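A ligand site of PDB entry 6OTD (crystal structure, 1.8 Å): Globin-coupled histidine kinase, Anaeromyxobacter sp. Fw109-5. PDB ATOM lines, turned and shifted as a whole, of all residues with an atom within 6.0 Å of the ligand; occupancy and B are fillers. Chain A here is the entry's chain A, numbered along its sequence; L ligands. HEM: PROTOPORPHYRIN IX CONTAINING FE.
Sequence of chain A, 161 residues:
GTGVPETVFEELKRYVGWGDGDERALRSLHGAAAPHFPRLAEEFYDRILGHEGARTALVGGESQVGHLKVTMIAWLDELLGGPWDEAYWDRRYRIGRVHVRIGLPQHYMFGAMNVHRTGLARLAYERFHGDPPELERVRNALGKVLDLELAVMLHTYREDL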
ATOM      1  N   PHE A  44       6.984 -10.018  -6.309  1.00  0.00           N
ATOM      2  CA  PHE A  44       6.994  -9.012  -5.252  1.00  0.00           C
ATOM      3  C   PHE A  44       8.207  -8.045  -5.378  1.00  0.00           C
ATOM      4  O   PHE A  44       8.096  -6.801  -5.266  1.00  0.00           O
ATOM      5  CB  PHE A  44       6.994  -9.764  -3.897  1.00  0.00           C
ATOM      6  CG  PHE A  44       6.801  -8.856  -2.711  1.00  0.00           C
ATOM      7  CD1 PHE A  44       7.878  -8.239  -2.146  1.00  0.00           C
ATOM      8  CD2 PHE A  44       5.522  -8.583  -2.218  1.00  0.00           C
ATOM      9  CE1 PHE A  44       7.707  -7.406  -1.049  1.00  0.00           C
ATOM     10  CE2 PHE A  44       5.345  -7.742  -1.124  1.00  0.00           C
ATOM     11  CZ  PHE A  44       6.444  -7.144  -0.545  1.00  0.00           C
ATOM     12  N   ILE A  48       8.703  -3.839  -6.197  1.00  0.00           N
ATOM     13  CA  ILE A  48       9.627  -2.937  -5.540  1.00  0.00           C
ATOM     14  C   ILE A  48      10.452  -2.172  -6.601  1.00  0.00           C
ATOM     15  O   ILE A  48      10.593  -0.926  -6.547  1.00  0.00           O
ATOM     16  CB  ILE A  48      10.556  -3.685  -4.550  1.00  0.00           C
ATOM     17  CG1 ILE A  48       9.736  -4.286  -3.372  1.00  0.00           C
ATOM     18  CG2 ILE A  48      11.677  -2.804  -4.069  1.00  0.00           C
ATOM     19  CD1 ILE A  48      10.574  -5.089  -2.402  1.00  0.00           C
ATOM     20  N   ALA A  54      10.264   2.843  -3.226  1.00  0.00           N
ATOM     21  CA  ALA A  54      10.625   1.590  -2.590  1.00  0.00           C
ATOM     22  C   ALA A  54      12.038   1.183  -3.043  1.00  0.00           C
ATOM     23  O   ALA A  54      12.826   0.701  -2.255  1.00  0.00           O
ATOM     24  CB  ALA A  54       9.636   0.495  -2.919  1.00  0.00           C
ATOM     25  N   ARG A  55      12.369   1.441  -4.304  1.00  0.00           N
ATOM     26  CA  ARG A  55      13.669   0.948  -4.751  1.00  0.00           C
ATOM     27  C   ARG A  55      14.877   1.637  -4.194  1.00  0.00           C
ATOM     28  O   ARG A  55      16.003   1.113  -4.319  1.00  0.00           O
ATOM     29  CB  ARG A  55      13.697   0.769  -6.277  1.00  0.00           C
ATOM     30  CG  ARG A  55      13.882   1.984  -7.101  1.00  0.00           C
ATOM     31  CD  ARG A  55      13.912   1.561  -8.578  1.00  0.00           C
ATOM     32  NE  ARG A  55      15.169   0.880  -8.973  1.00  0.00           N
ATOM     33  CZ  ARG A  55      15.323   0.062 -10.024  1.00  0.00           C
ATOM     34  NH1 ARG A  55      16.514  -0.438 -10.293  1.00  0.00           N
ATOM     35  NH2 ARG A  55      14.289  -0.274 -10.824  1.00  0.00           N
ATOM     36  N   ALA A  57      15.560   1.596  -1.225  1.00  0.00           N
ATOM     37  CA  ALA A  57      16.131   0.686  -0.175  1.00  0.00           C
ATOM     38  C   ALA A  57      17.187  -0.301  -0.722  1.00  0.00           C
ATOM     39  O   ALA A  57      17.888  -0.972   0.049  1.00  0.00           O
ATOM     40  CB  ALA A  57      15.030  -0.106   0.472  1.00  0.00           C
ATOM     41  N   LEU A  58      17.289  -0.402  -2.037  1.00  0.00           N
ATOM     42  CA  LEU A  58      18.082  -1.445  -2.668  1.00  0.00           C
ATOM     43  C   LEU A  58      19.483  -0.928  -2.852  1.00  0.00           C
ATOM     44  O   LEU A  58      19.961  -0.743  -3.983  1.00  0.00           O
ATOM     45  CB  LEU A  58      17.485  -1.940  -4.014  1.00  0.00           C
ATOM     46  CG  LEU A  58      16.040  -2.408  -3.942  1.00  0.00           C
ATOM     47  CD1 LEU A  58      15.569  -2.839  -5.317  1.00  0.00           C
ATOM     48  CD2 LEU A  58      15.872  -3.537  -2.916  1.00  0.00           C
ATOM     49  N   SER A  63      24.159  -9.183  -3.504  1.00  0.00           N
ATOM     50  CA  SER A  63      23.798 -10.055  -2.392  1.00  0.00           C
ATOM     51  C   SER A  63      22.389  -9.725  -1.833  1.00  0.00           C
ATOM     52  O   SER A  63      21.656 -10.607  -1.391  1.00  0.00           O
ATOM     53  CB  SER A  63      24.806  -9.906  -1.254  1.00  0.00           C
ATOM     54  OG  SER A  63      26.092 -10.325  -1.632  1.00  0.00           O
ATOM     55  N   GLN A  64      22.050  -8.450  -1.843  1.00  0.00           N
ATOM     56  CA  GLN A  64      20.757  -8.027  -1.314  1.00  0.00           C
ATOM     57  C   GLN A  64      19.613  -8.607  -2.144  1.00  0.00           C
ATOM     58  O   GLN A  64      18.574  -8.973  -1.579  1.00  0.00           O
ATOM     59  CB  GLN A  64      20.636  -6.513  -1.191  1.00  0.00           C
ATOM     60  CG  GLN A  64      19.232  -6.029  -0.747  1.00  0.00           C
ATOM     61  CD  GLN A  64      19.180  -4.532  -0.708  1.00  0.00           C
ATOM     62  OE1 GLN A  64      19.726  -3.852  -1.637  1.00  0.00           O
ATOM     63  NE2 GLN A  64      18.426  -3.990   0.276  1.00  0.00           N
ATOM     64  N   VAL A  65      19.825  -8.721  -3.458  1.00  0.00           N
ATOM     65  CA  VAL A  65      18.775  -9.189  -4.331  1.00  0.00           C
ATOM     66  C   VAL A  65      18.372 -10.634  -3.933  1.00  0.00           C
ATOM     67  O   VAL A  65      17.162 -10.953  -3.772  1.00  0.00           O
ATOM     68  CB  VAL A  65      19.190  -9.156  -5.815  1.00  0.00           C
ATOM     69  CG1 VAL A  65      18.099  -9.769  -6.704  1.00  0.00           C
ATOM     70  CG2 VAL A  65      19.523  -7.697  -6.217  1.00  0.00           C
ATOM     71  N   HIS A  67      18.955 -12.036  -1.076  1.00  0.00           N
ATOM     72  CA  HIS A  67      18.448 -12.025   0.307  1.00  0.00           C
ATOM     73  C   HIS A  67      16.957 -11.659   0.359  1.00  0.00           C
ATOM     74  O   HIS A  67      16.207 -12.287   1.054  1.00  0.00           O
ATOM     75  CB  HIS A  67      19.227 -11.135   1.205  1.00  0.00           C
ATOM     76  CG  HIS A  67      18.879 -11.323   2.645  1.00  0.00           C
ATOM     77  ND1 HIS A  67      18.291 -10.338   3.408  1.00  0.00           N
ATOM     78  CD2 HIS A  67      18.991 -12.410   3.439  1.00  0.00           C
ATOM     79  CE1 HIS A  67      18.124 -10.795   4.632  1.00  0.00           C
ATOM     80  NE2 HIS A  67      18.496 -12.054   4.664  1.00  0.00           N
ATOM     81  N   LEU A  68      16.552 -10.666  -0.420  1.00  0.00           N
ATOM     82  CA  LEU A  68      15.122 -10.261  -0.538  1.00  0.00           C
ATOM     83  C   LEU A  68      14.263 -11.396  -1.083  1.00  0.00           C
ATOM     84  O   LEU A  68      13.091 -11.532  -0.696  1.00  0.00           O
ATOM     85  CB  LEU A  68      14.990  -9.017  -1.385  1.00  0.00           C
ATOM     86  CG  LEU A  68      15.601  -7.782  -0.659  1.00  0.00           C
ATOM     87  CD1 LEU A  68      15.676  -6.587  -1.594  1.00  0.00           C
ATOM     88  CD2 LEU A  68      14.833  -7.446   0.655  1.00  0.00           C
ATOM     89  N   THR A  71      14.215 -14.402   1.831  1.00  0.00           N
ATOM     90  CA  THR A  71      13.442 -13.965   2.960  1.00  0.00           C
ATOM     91  C   THR A  71      11.949 -14.020   2.699  1.00  0.00           C
ATOM     92  O   THR A  71      11.135 -14.377   3.566  1.00  0.00           O
ATOM     93  CB  THR A  71      13.852 -12.541   3.444  1.00  0.00           C
ATOM     94  OG1 THR A  71      13.908 -11.605   2.361  1.00  0.00           O
ATOM     95  CG2 THR A  71      15.207 -12.628   4.152  1.00  0.00           C
ATOM     96  N   MET A  72      11.570 -13.634   1.514  1.00  0.00           N
ATOM     97  CA  MET A  72      10.164 -13.645   1.165  1.00  0.00           C
ATOM     98  C   MET A  72       9.652 -15.056   0.943  1.00  0.00           C
ATOM     99  O   MET A  72       8.497 -15.351   1.223  1.00  0.00           O
ATOM    100  CB  MET A  72       9.937 -12.775  -0.039  1.00  0.00           C
ATOM    101  CG  MET A  72       8.496 -12.594  -0.414  1.00  0.00           C
ATOM    102  SD  MET A  72       7.557 -11.858   0.956  1.00  0.00           S
ATOM    103  CE  MET A  72       8.272 -10.234   1.058  1.00  0.00           C
ATOM    104  N   TRP A  75       9.178 -16.377   4.357  1.00  0.00           N
ATOM    105  CA  TRP A  75       8.002 -15.718   4.949  1.00  0.00           C
ATOM    106  C   TRP A  75       6.685 -16.378   4.482  1.00  0.00           C
ATOM    107  O   TRP A  75       5.820 -16.688   5.288  1.00  0.00           O
ATOM    108  CB  TRP A  75       7.993 -14.230   4.543  1.00  0.00           C
ATOM    109  CG  TRP A  75       6.858 -13.437   5.234  1.00  0.00           C
ATOM    110  CD1 TRP A  75       6.885 -12.922   6.441  1.00  0.00           C
ATOM    111  CD2 TRP A  75       5.615 -13.128   4.678  1.00  0.00           C
ATOM    112  NE1 TRP A  75       5.738 -12.260   6.693  1.00  0.00           N
ATOM    113  CE2 TRP A  75       4.912 -12.385   5.637  1.00  0.00           C
ATOM    114  CE3 TRP A  75       5.038 -13.343   3.431  1.00  0.00           C
ATOM    115  CZ2 TRP A  75       3.630 -11.886   5.420  1.00  0.00           C
ATOM    116  CZ3 TRP A  75       3.717 -12.825   3.199  1.00  0.00           C
ATOM    117  CH2 TRP A  75       3.042 -12.107   4.217  1.00  0.00           C
ATOM    118  N   ARG A  94       9.491  -8.778  15.075  1.00  0.00           N
ATOM    119  CA  ARG A  94      10.897  -8.509  14.686  1.00  0.00           C
ATOM    120  C   ARG A  94      11.067  -8.146  13.192  1.00  0.00           C
ATOM    121  O   ARG A  94      11.770  -7.202  12.857  1.00  0.00           O
ATOM    122  CB  ARG A  94      11.761  -9.688  15.029  1.00  0.00           C
ATOM    123  CG  ARG A  94      11.993  -9.875  16.538  1.00  0.00           C
ATOM    124  CD  ARG A  94      13.130 -10.853  16.854  1.00  0.00           C
ATOM    125  NE  ARG A  94      12.671 -12.238  16.961  1.00  0.00           N
ATOM    126  CZ  ARG A  94      11.916 -12.742  17.949  1.00  0.00           C
ATOM    127  NH1 ARG A  94      11.501 -11.992  18.985  1.00  0.00           N
ATOM    128  NH2 ARG A  94      11.559 -14.032  17.901  1.00  0.00           N
ATOM    129  N   ILE A  95      10.404  -8.877  12.316  1.00  0.00           N
ATOM    130  CA  ILE A  95      10.393  -8.534  10.871  1.00  0.00           C
ATOM    131  C   ILE A  95       9.877  -7.132  10.650  1.00  0.00           C
ATOM    132  O   ILE A  95      10.427  -6.336   9.848  1.00  0.00           O
ATOM    133  CB  ILE A  95       9.582  -9.586  10.086  1.00  0.00           C
ATOM    134  CG1 ILE A  95      10.420 -10.888  10.009  1.00  0.00           C
ATOM    135  CG2 ILE A  95       9.238  -9.074   8.665  1.00  0.00           C
ATOM    136  CD1 ILE A  95       9.646 -12.149   9.758  1.00  0.00           C
ATOM    137  N   VAL A  98      12.415  -4.468  11.544  1.00  0.00           N
ATOM    138  CA  VAL A  98      13.490  -4.330  10.568  1.00  0.00           C
ATOM    139  C   VAL A  98      13.097  -3.278   9.551  1.00  0.00           C
ATOM    140  O   VAL A  98      13.894  -2.381   9.259  1.00  0.00           O
ATOM    141  CB  VAL A  98      13.817  -5.696   9.867  1.00  0.00           C
ATOM    142  CG1 VAL A  98      14.619  -5.480   8.614  1.00  0.00           C
ATOM    143  CG2 VAL A  98      14.537  -6.642  10.834  1.00  0.00           C
ATOM    144  N   HIS A  99      11.855  -3.312   9.052  1.00  0.00           N
ATOM    145  CA  HIS A  99      11.452  -2.307   8.066  1.00  0.00           C
ATOM    146  C   HIS A  99      11.360  -0.902   8.662  1.00  0.00           C
ATOM    147  O   HIS A  99      11.669   0.107   7.987  1.00  0.00           O
ATOM    148  CB  HIS A  99      10.143  -2.644   7.416  1.00  0.00           C
ATOM    149  CG  HIS A  99      10.196  -3.969   6.724  1.00  0.00           C
ATOM    150  ND1 HIS A  99      10.052  -5.149   7.414  1.00  0.00           N
ATOM    151  CD2 HIS A  99      10.500  -4.283   5.445  1.00  0.00           C
ATOM    152  CE1 HIS A  99      10.226  -6.154   6.562  1.00  0.00           C
ATOM    153  NE2 HIS A  99      10.466  -5.652   5.366  1.00  0.00           N
ATOM    154  N   ILE A 102      14.973   0.569   9.030  1.00  0.00           N
ATOM    155  CA  ILE A 102      15.606   1.091   7.804  1.00  0.00           C
ATOM    156  C   ILE A 102      14.863   2.226   7.135  1.00  0.00           C
ATOM    157  O   ILE A 102      15.339   2.766   6.149  1.00  0.00           O
ATOM    158  CB  ILE A 102      15.967  -0.023   6.794  1.00  0.00           C
ATOM    159  CG1 ILE A 102      14.724  -0.563   6.111  1.00  0.00           C
ATOM    160  CG2 ILE A 102      16.831  -1.085   7.476  1.00  0.00           C
ATOM    161  CD1 ILE A 102      14.872  -2.009   5.626  1.00  0.00           C
ATOM    162  N   LEU A 104      11.531   2.529   5.965  1.00  0.00           N
ATOM    163  CA  LEU A 104      10.509   2.345   4.986  1.00  0.00           C
ATOM    164  C   LEU A 104       9.248   2.938   5.547  1.00  0.00           C
ATOM    165  O   LEU A 104       8.909   2.595   6.672  1.00  0.00           O
ATOM    166  CB  LEU A 104      10.291   0.857   4.679  1.00  0.00           C
ATOM    167  CG  LEU A 104      11.469   0.252   3.936  1.00  0.00           C
ATOM    168  CD1 LEU A 104      11.270  -1.254   3.810  1.00  0.00           C
ATOM    169  CD2 LEU A 104      11.633   0.897   2.560  1.00  0.00           C
ATOM    170  N   TYR A 108       3.720   1.875   2.424  1.00  0.00           N
ATOM    171  CA  TYR A 108       4.185   0.839   1.482  1.00  0.00           C
ATOM    172  C   TYR A 108       3.660  -0.551   1.839  1.00  0.00           C
ATOM    173  O   TYR A 108       3.531  -1.408   0.960  1.00  0.00           O
ATOM    174  CB  TYR A 108       5.725   0.746   1.484  1.00  0.00           C
ATOM    175  CG  TYR A 108       6.488   1.905   0.822  1.00  0.00           C
ATOM    176  CD1 TYR A 108       5.837   3.039   0.354  1.00  0.00           C
ATOM    177  CD2 TYR A 108       7.896   1.878   0.719  1.00  0.00           C
ATOM    178  CE1 TYR A 108       6.544   4.093  -0.240  1.00  0.00           C
ATOM    179  CE2 TYR A 108       8.598   2.940   0.123  1.00  0.00           C
ATOM    180  CZ  TYR A 108       7.902   4.026  -0.361  1.00  0.00           C
ATOM    181  OH  TYR A 108       8.536   5.101  -0.932  1.00  0.00           O
ATOM    182  N   MET A 109       3.436  -0.792   3.122  1.00  0.00           N
ATOM    183  CA  MET A 109       2.997  -2.090   3.548  1.00  0.00           C
ATOM    184  C   MET A 109       1.593  -2.416   3.067  1.00  0.00           C
ATOM    185  O   MET A 109       1.269  -3.600   2.846  1.00  0.00           O
ATOM    186  CB  MET A 109       3.168  -2.250   5.037  1.00  0.00           C
ATOM    187  CG  MET A 109       4.572  -2.035   5.565  1.00  0.00           C
ATOM    188  SD  MET A 109       5.766  -3.104   4.696  1.00  0.00           S
ATOM    189  CE  MET A 109       7.118  -3.139   5.859  1.00  0.00           C
ATOM    190  N   ALA A 112       2.089  -3.572  -0.429  1.00  0.00           N
ATOM    191  CA  ALA A 112       2.815  -4.801  -0.390  1.00  0.00           C
ATOM    192  C   ALA A 112       1.937  -5.976   0.028  1.00  0.00           C
ATOM    193  O   ALA A 112       2.026  -7.057  -0.561  1.00  0.00           O
ATOM    194  CB  ALA A 112       4.038  -4.692   0.513  1.00  0.00           C
ATOM    195  N   MET A 113       1.047  -5.766   0.998  1.00  0.00           N
ATOM    196  CA  MET A 113       0.143  -6.829   1.388  1.00  0.00           C
ATOM    197  C   MET A 113      -0.856  -7.079   0.266  1.00  0.00           C
ATOM    198  O   MET A 113      -1.200  -8.220   0.025  1.00  0.00           O
ATOM    199  CB  MET A 113      -0.562  -6.510   2.713  1.00  0.00           C
ATOM    200  CG  MET A 113       0.402  -6.652   3.854  1.00  0.00           C
ATOM    201  SD  MET A 113       0.787  -8.403   4.161  1.00  0.00           S
ATOM    202  CE  MET A 113       1.926  -8.263   5.507  1.00  0.00           C
ATOM    203  N   HIS A 116       0.455  -9.688  -2.173  1.00  0.00           N
ATOM    204  CA  HIS A 116       0.286 -11.045  -1.679  1.00  0.00           C
ATOM    205  C   HIS A 116      -1.155 -11.509  -1.644  1.00  0.00           C
ATOM    206  O   HIS A 116      -1.468 -12.696  -1.900  1.00  0.00           O
ATOM    207  CB  HIS A 116       0.869 -11.138  -0.273  1.00  0.00           C
ATOM    208  CG  HIS A 116       2.357 -11.152  -0.267  1.00  0.00           C
ATOM    209  ND1 HIS A 116       3.077 -12.016  -1.050  1.00  0.00           N
ATOM    210  CD2 HIS A 116       3.266 -10.490   0.494  1.00  0.00           C
ATOM    211  CE1 HIS A 116       4.365 -11.846  -0.817  1.00  0.00           C
ATOM    212  NE2 HIS A 116       4.508 -10.919   0.099  1.00  0.00           N
ATOM    213  N   GLU A 149      -1.108 -10.264   9.820  1.00  0.00           N
ATOM    214  CA  GLU A 149       0.237  -9.879   9.411  1.00  0.00           C
ATOM    215  C   GLU A 149       0.354  -8.364   9.262  1.00  0.00           C
ATOM    216  O   GLU A 149       1.245  -7.789   9.779  1.00  0.00           O
ATOM    217  CB  GLU A 149       0.655 -10.544   8.080  1.00  0.00           C
ATOM    218  CG  GLU A 149       0.896 -12.036   8.208  1.00  0.00           C
ATOM    219  CD  GLU A 149       2.255 -12.393   8.759  1.00  0.00           C
ATOM    220  OE1 GLU A 149       2.518 -13.608   8.929  1.00  0.00           O
ATOM    221  OE2 GLU A 149       3.057 -11.482   8.947  1.00  0.00           O
ATOM    222  N   MET A 153       2.667  -5.893  11.598  1.00  0.00           N
ATOM    223  CA  MET A 153       3.726  -5.102  10.953  1.00  0.00           C
ATOM    224  C   MET A 153       3.512  -3.629  11.270  1.00  0.00           C
ATOM    225  O   MET A 153       4.430  -2.950  11.620  1.00  0.00           O
ATOM    226  CB  MET A 153       3.741  -5.262   9.436  1.00  0.00           C
ATOM    227  CG  MET A 153       4.834  -4.461   8.713  1.00  0.00           C
ATOM    228  SD  MET A 153       6.213  -5.475   8.138  1.00  0.00           S
ATOM    229  CE  MET A 153       5.897  -6.998   9.061  1.00  0.00           C
HETATM  230  CHA HEM L   1      13.714  -7.613   5.261  1.00  0.00           C
HETATM  231  CHB HEM L   1       9.316  -9.429   4.768  1.00  0.00           C
HETATM  232  CHC HEM L   1       7.963  -5.397   2.554  1.00  0.00           C
HETATM  233  CHD HEM L   1      12.551  -4.232   2.058  1.00  0.00           C
HETATM  234  C1A HEM L   1      12.638  -8.405   5.334  1.00  0.00           C
HETATM  235  C2A HEM L   1      12.685  -9.674   5.922  1.00  0.00           C
HETATM  236  C3A HEM L   1      11.443 -10.212   5.808  1.00  0.00           C
HETATM  237  C4A HEM L   1      10.648  -9.270   5.111  1.00  0.00           C
HETATM  238  CMA HEM L   1      10.985 -11.608   6.283  1.00  0.00           C
HETATM  239  CAA HEM L   1      13.913 -10.272   6.622  1.00  0.00           C
HETATM  240  CBA HEM L   1      13.834  -9.804   8.068  1.00  0.00           C
HETATM  241  CGA HEM L   1      14.894 -10.326   9.059  1.00  0.00           C
HETATM  242  O1A HEM L   1      16.044  -9.913   8.971  1.00  0.00           O
HETATM  243  O2A HEM L   1      14.658 -11.101  10.011  1.00  0.00           O
HETATM  244  C1B HEM L   1       8.518  -8.475   4.199  1.00  0.00           C
HETATM  245  C2B HEM L   1       7.085  -8.589   4.060  1.00  0.00           C
HETATM  246  C3B HEM L   1       6.685  -7.403   3.450  1.00  0.00           C
HETATM  247  C4B HEM L   1       7.912  -6.617   3.191  1.00  0.00           C
HETATM  248  CMB HEM L   1       6.280  -9.781   4.542  1.00  0.00           C
HETATM  249  CAB HEM L   1       5.334  -6.939   3.029  1.00  0.00           C
HETATM  250  CBB HEM L   1       4.280  -7.703   3.062  1.00  0.00           C
HETATM  251  C1C HEM L   1       9.055  -4.709   2.149  1.00  0.00           C
HETATM  252  C2C HEM L   1       9.060  -3.597   1.260  1.00  0.00           C
HETATM  253  C3C HEM L   1      10.389  -3.305   1.076  1.00  0.00           C
HETATM  254  C4C HEM L   1      11.183  -4.204   1.872  1.00  0.00           C
HETATM  255  CMC HEM L   1       7.845  -2.966   0.598  1.00  0.00           C
HETATM  256  CAC HEM L   1      10.769  -2.221   0.166  1.00  0.00           C
HETATM  257  CBC HEM L   1      11.972  -2.099  -0.338  1.00  0.00           C
HETATM  258  C1D HEM L   1      13.210  -5.027   2.961  1.00  0.00           C
HETATM  259  C2D HEM L   1      14.642  -4.852   3.260  1.00  0.00           C
HETATM  260  C3D HEM L   1      14.956  -5.791   4.169  1.00  0.00           C
HETATM  261  C4D HEM L   1      13.705  -6.544   4.388  1.00  0.00           C
HETATM  262  CMD HEM L   1      15.477  -3.737   2.624  1.00  0.00           C
HETATM  263  CAD HEM L   1      16.317  -6.043   4.814  1.00  0.00           C
HETATM  264  CBD HEM L   1      17.126  -7.211   4.184  1.00  0.00           C
HETATM  265  CGD HEM L   1      17.716  -6.976   2.806  1.00  0.00           C
HETATM  266  O1D HEM L   1      17.809  -5.837   2.339  1.00  0.00           O
HETATM  267  O2D HEM L   1      18.177  -7.969   2.132  1.00  0.00           O
HETATM  268  NA  HEM L   1      11.391  -8.205   4.796  1.00  0.00           N
HETATM  269  NB  HEM L   1       8.903  -7.332   3.627  1.00  0.00           N
HETATM  270  NC  HEM L   1      10.338  -5.091   2.419  1.00  0.00           N
HETATM  271  ND  HEM L   1      12.691  -6.102   3.640  1.00  0.00           N
HETATM  272 FE   HEM L   1      10.867  -6.683   3.612  1.00  0.00          FE
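NE2 of Gln 64 is in hydrogen-bond range of O1D of the ligand (2.8 Å).
An oxygen (O2D) of the ligand sits at hydrogen-bond distance from a ring nitrogen (ND1) of His 67, at 2.7 Å.
FE of the ligand is bound by NE2 of His 99, 2.1 Å away.
The backbone carbonyl oxygen (O) of Leu 68 sits at hydrogen-bond distance from the side-chain hydroxyl (OG1) of Thr 71, at 3.2 Å.
The side-chain sulfur (SD) of Met 72 lies within hydrogen-bond range of a ring nitrogen (NE2) of His 116.
NE2 of Gln 64 is in hydrogen-bond range of O of Ala 57 (3.1 Å).
A ring nitrogen (ND1) of His 99 sits at hydrogen-bond distance from the backbone carbonyl oxygen (O) of Ile 95 (2.7 Å).
The backbone carbonyl oxygen (O) of His 99 sits at hydrogen-bond distance from the backbone NH (N) of Leu 104 (3.2 Å).
The side-chain hydroxyl (OG1) of Thr 71 lies within hydrogen-bond range of the backbone carbonyl oxygen (O) of His 67 (2.7 Å).
Residues that only touch the ligand: Trp 75, Met 113, Ala 54, Ile 102, Leu 104, Met 72, Ala 112, Leu 68, Thr 71, Ala 57, Phe 44, Ile 95, Ile 48, Met 109 and His 116.
Hydrophobic or aromatic side chains that line the ligand: Phe 44, Ile 48, Ala 57, His 67, Leu 68, Met 72, Trp 75, Ile 95, His 99, Ile 102, Leu 104, Met 109, Ala 112, Met 113 and His 116.
Within 4 Å of the ligand: Phe 44, Ile 48, Ala 54, Ala 57, Gln 64, His 67, Leu 68, Thr 71, Met 72, Trp 75, Ile 95, His 99, Ile 102, Leu 104, Met 109, Ala 112, Met 113 and His 116.
The nearest printed residue that does not touch the ligand is Val 98 (4.1 Å).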
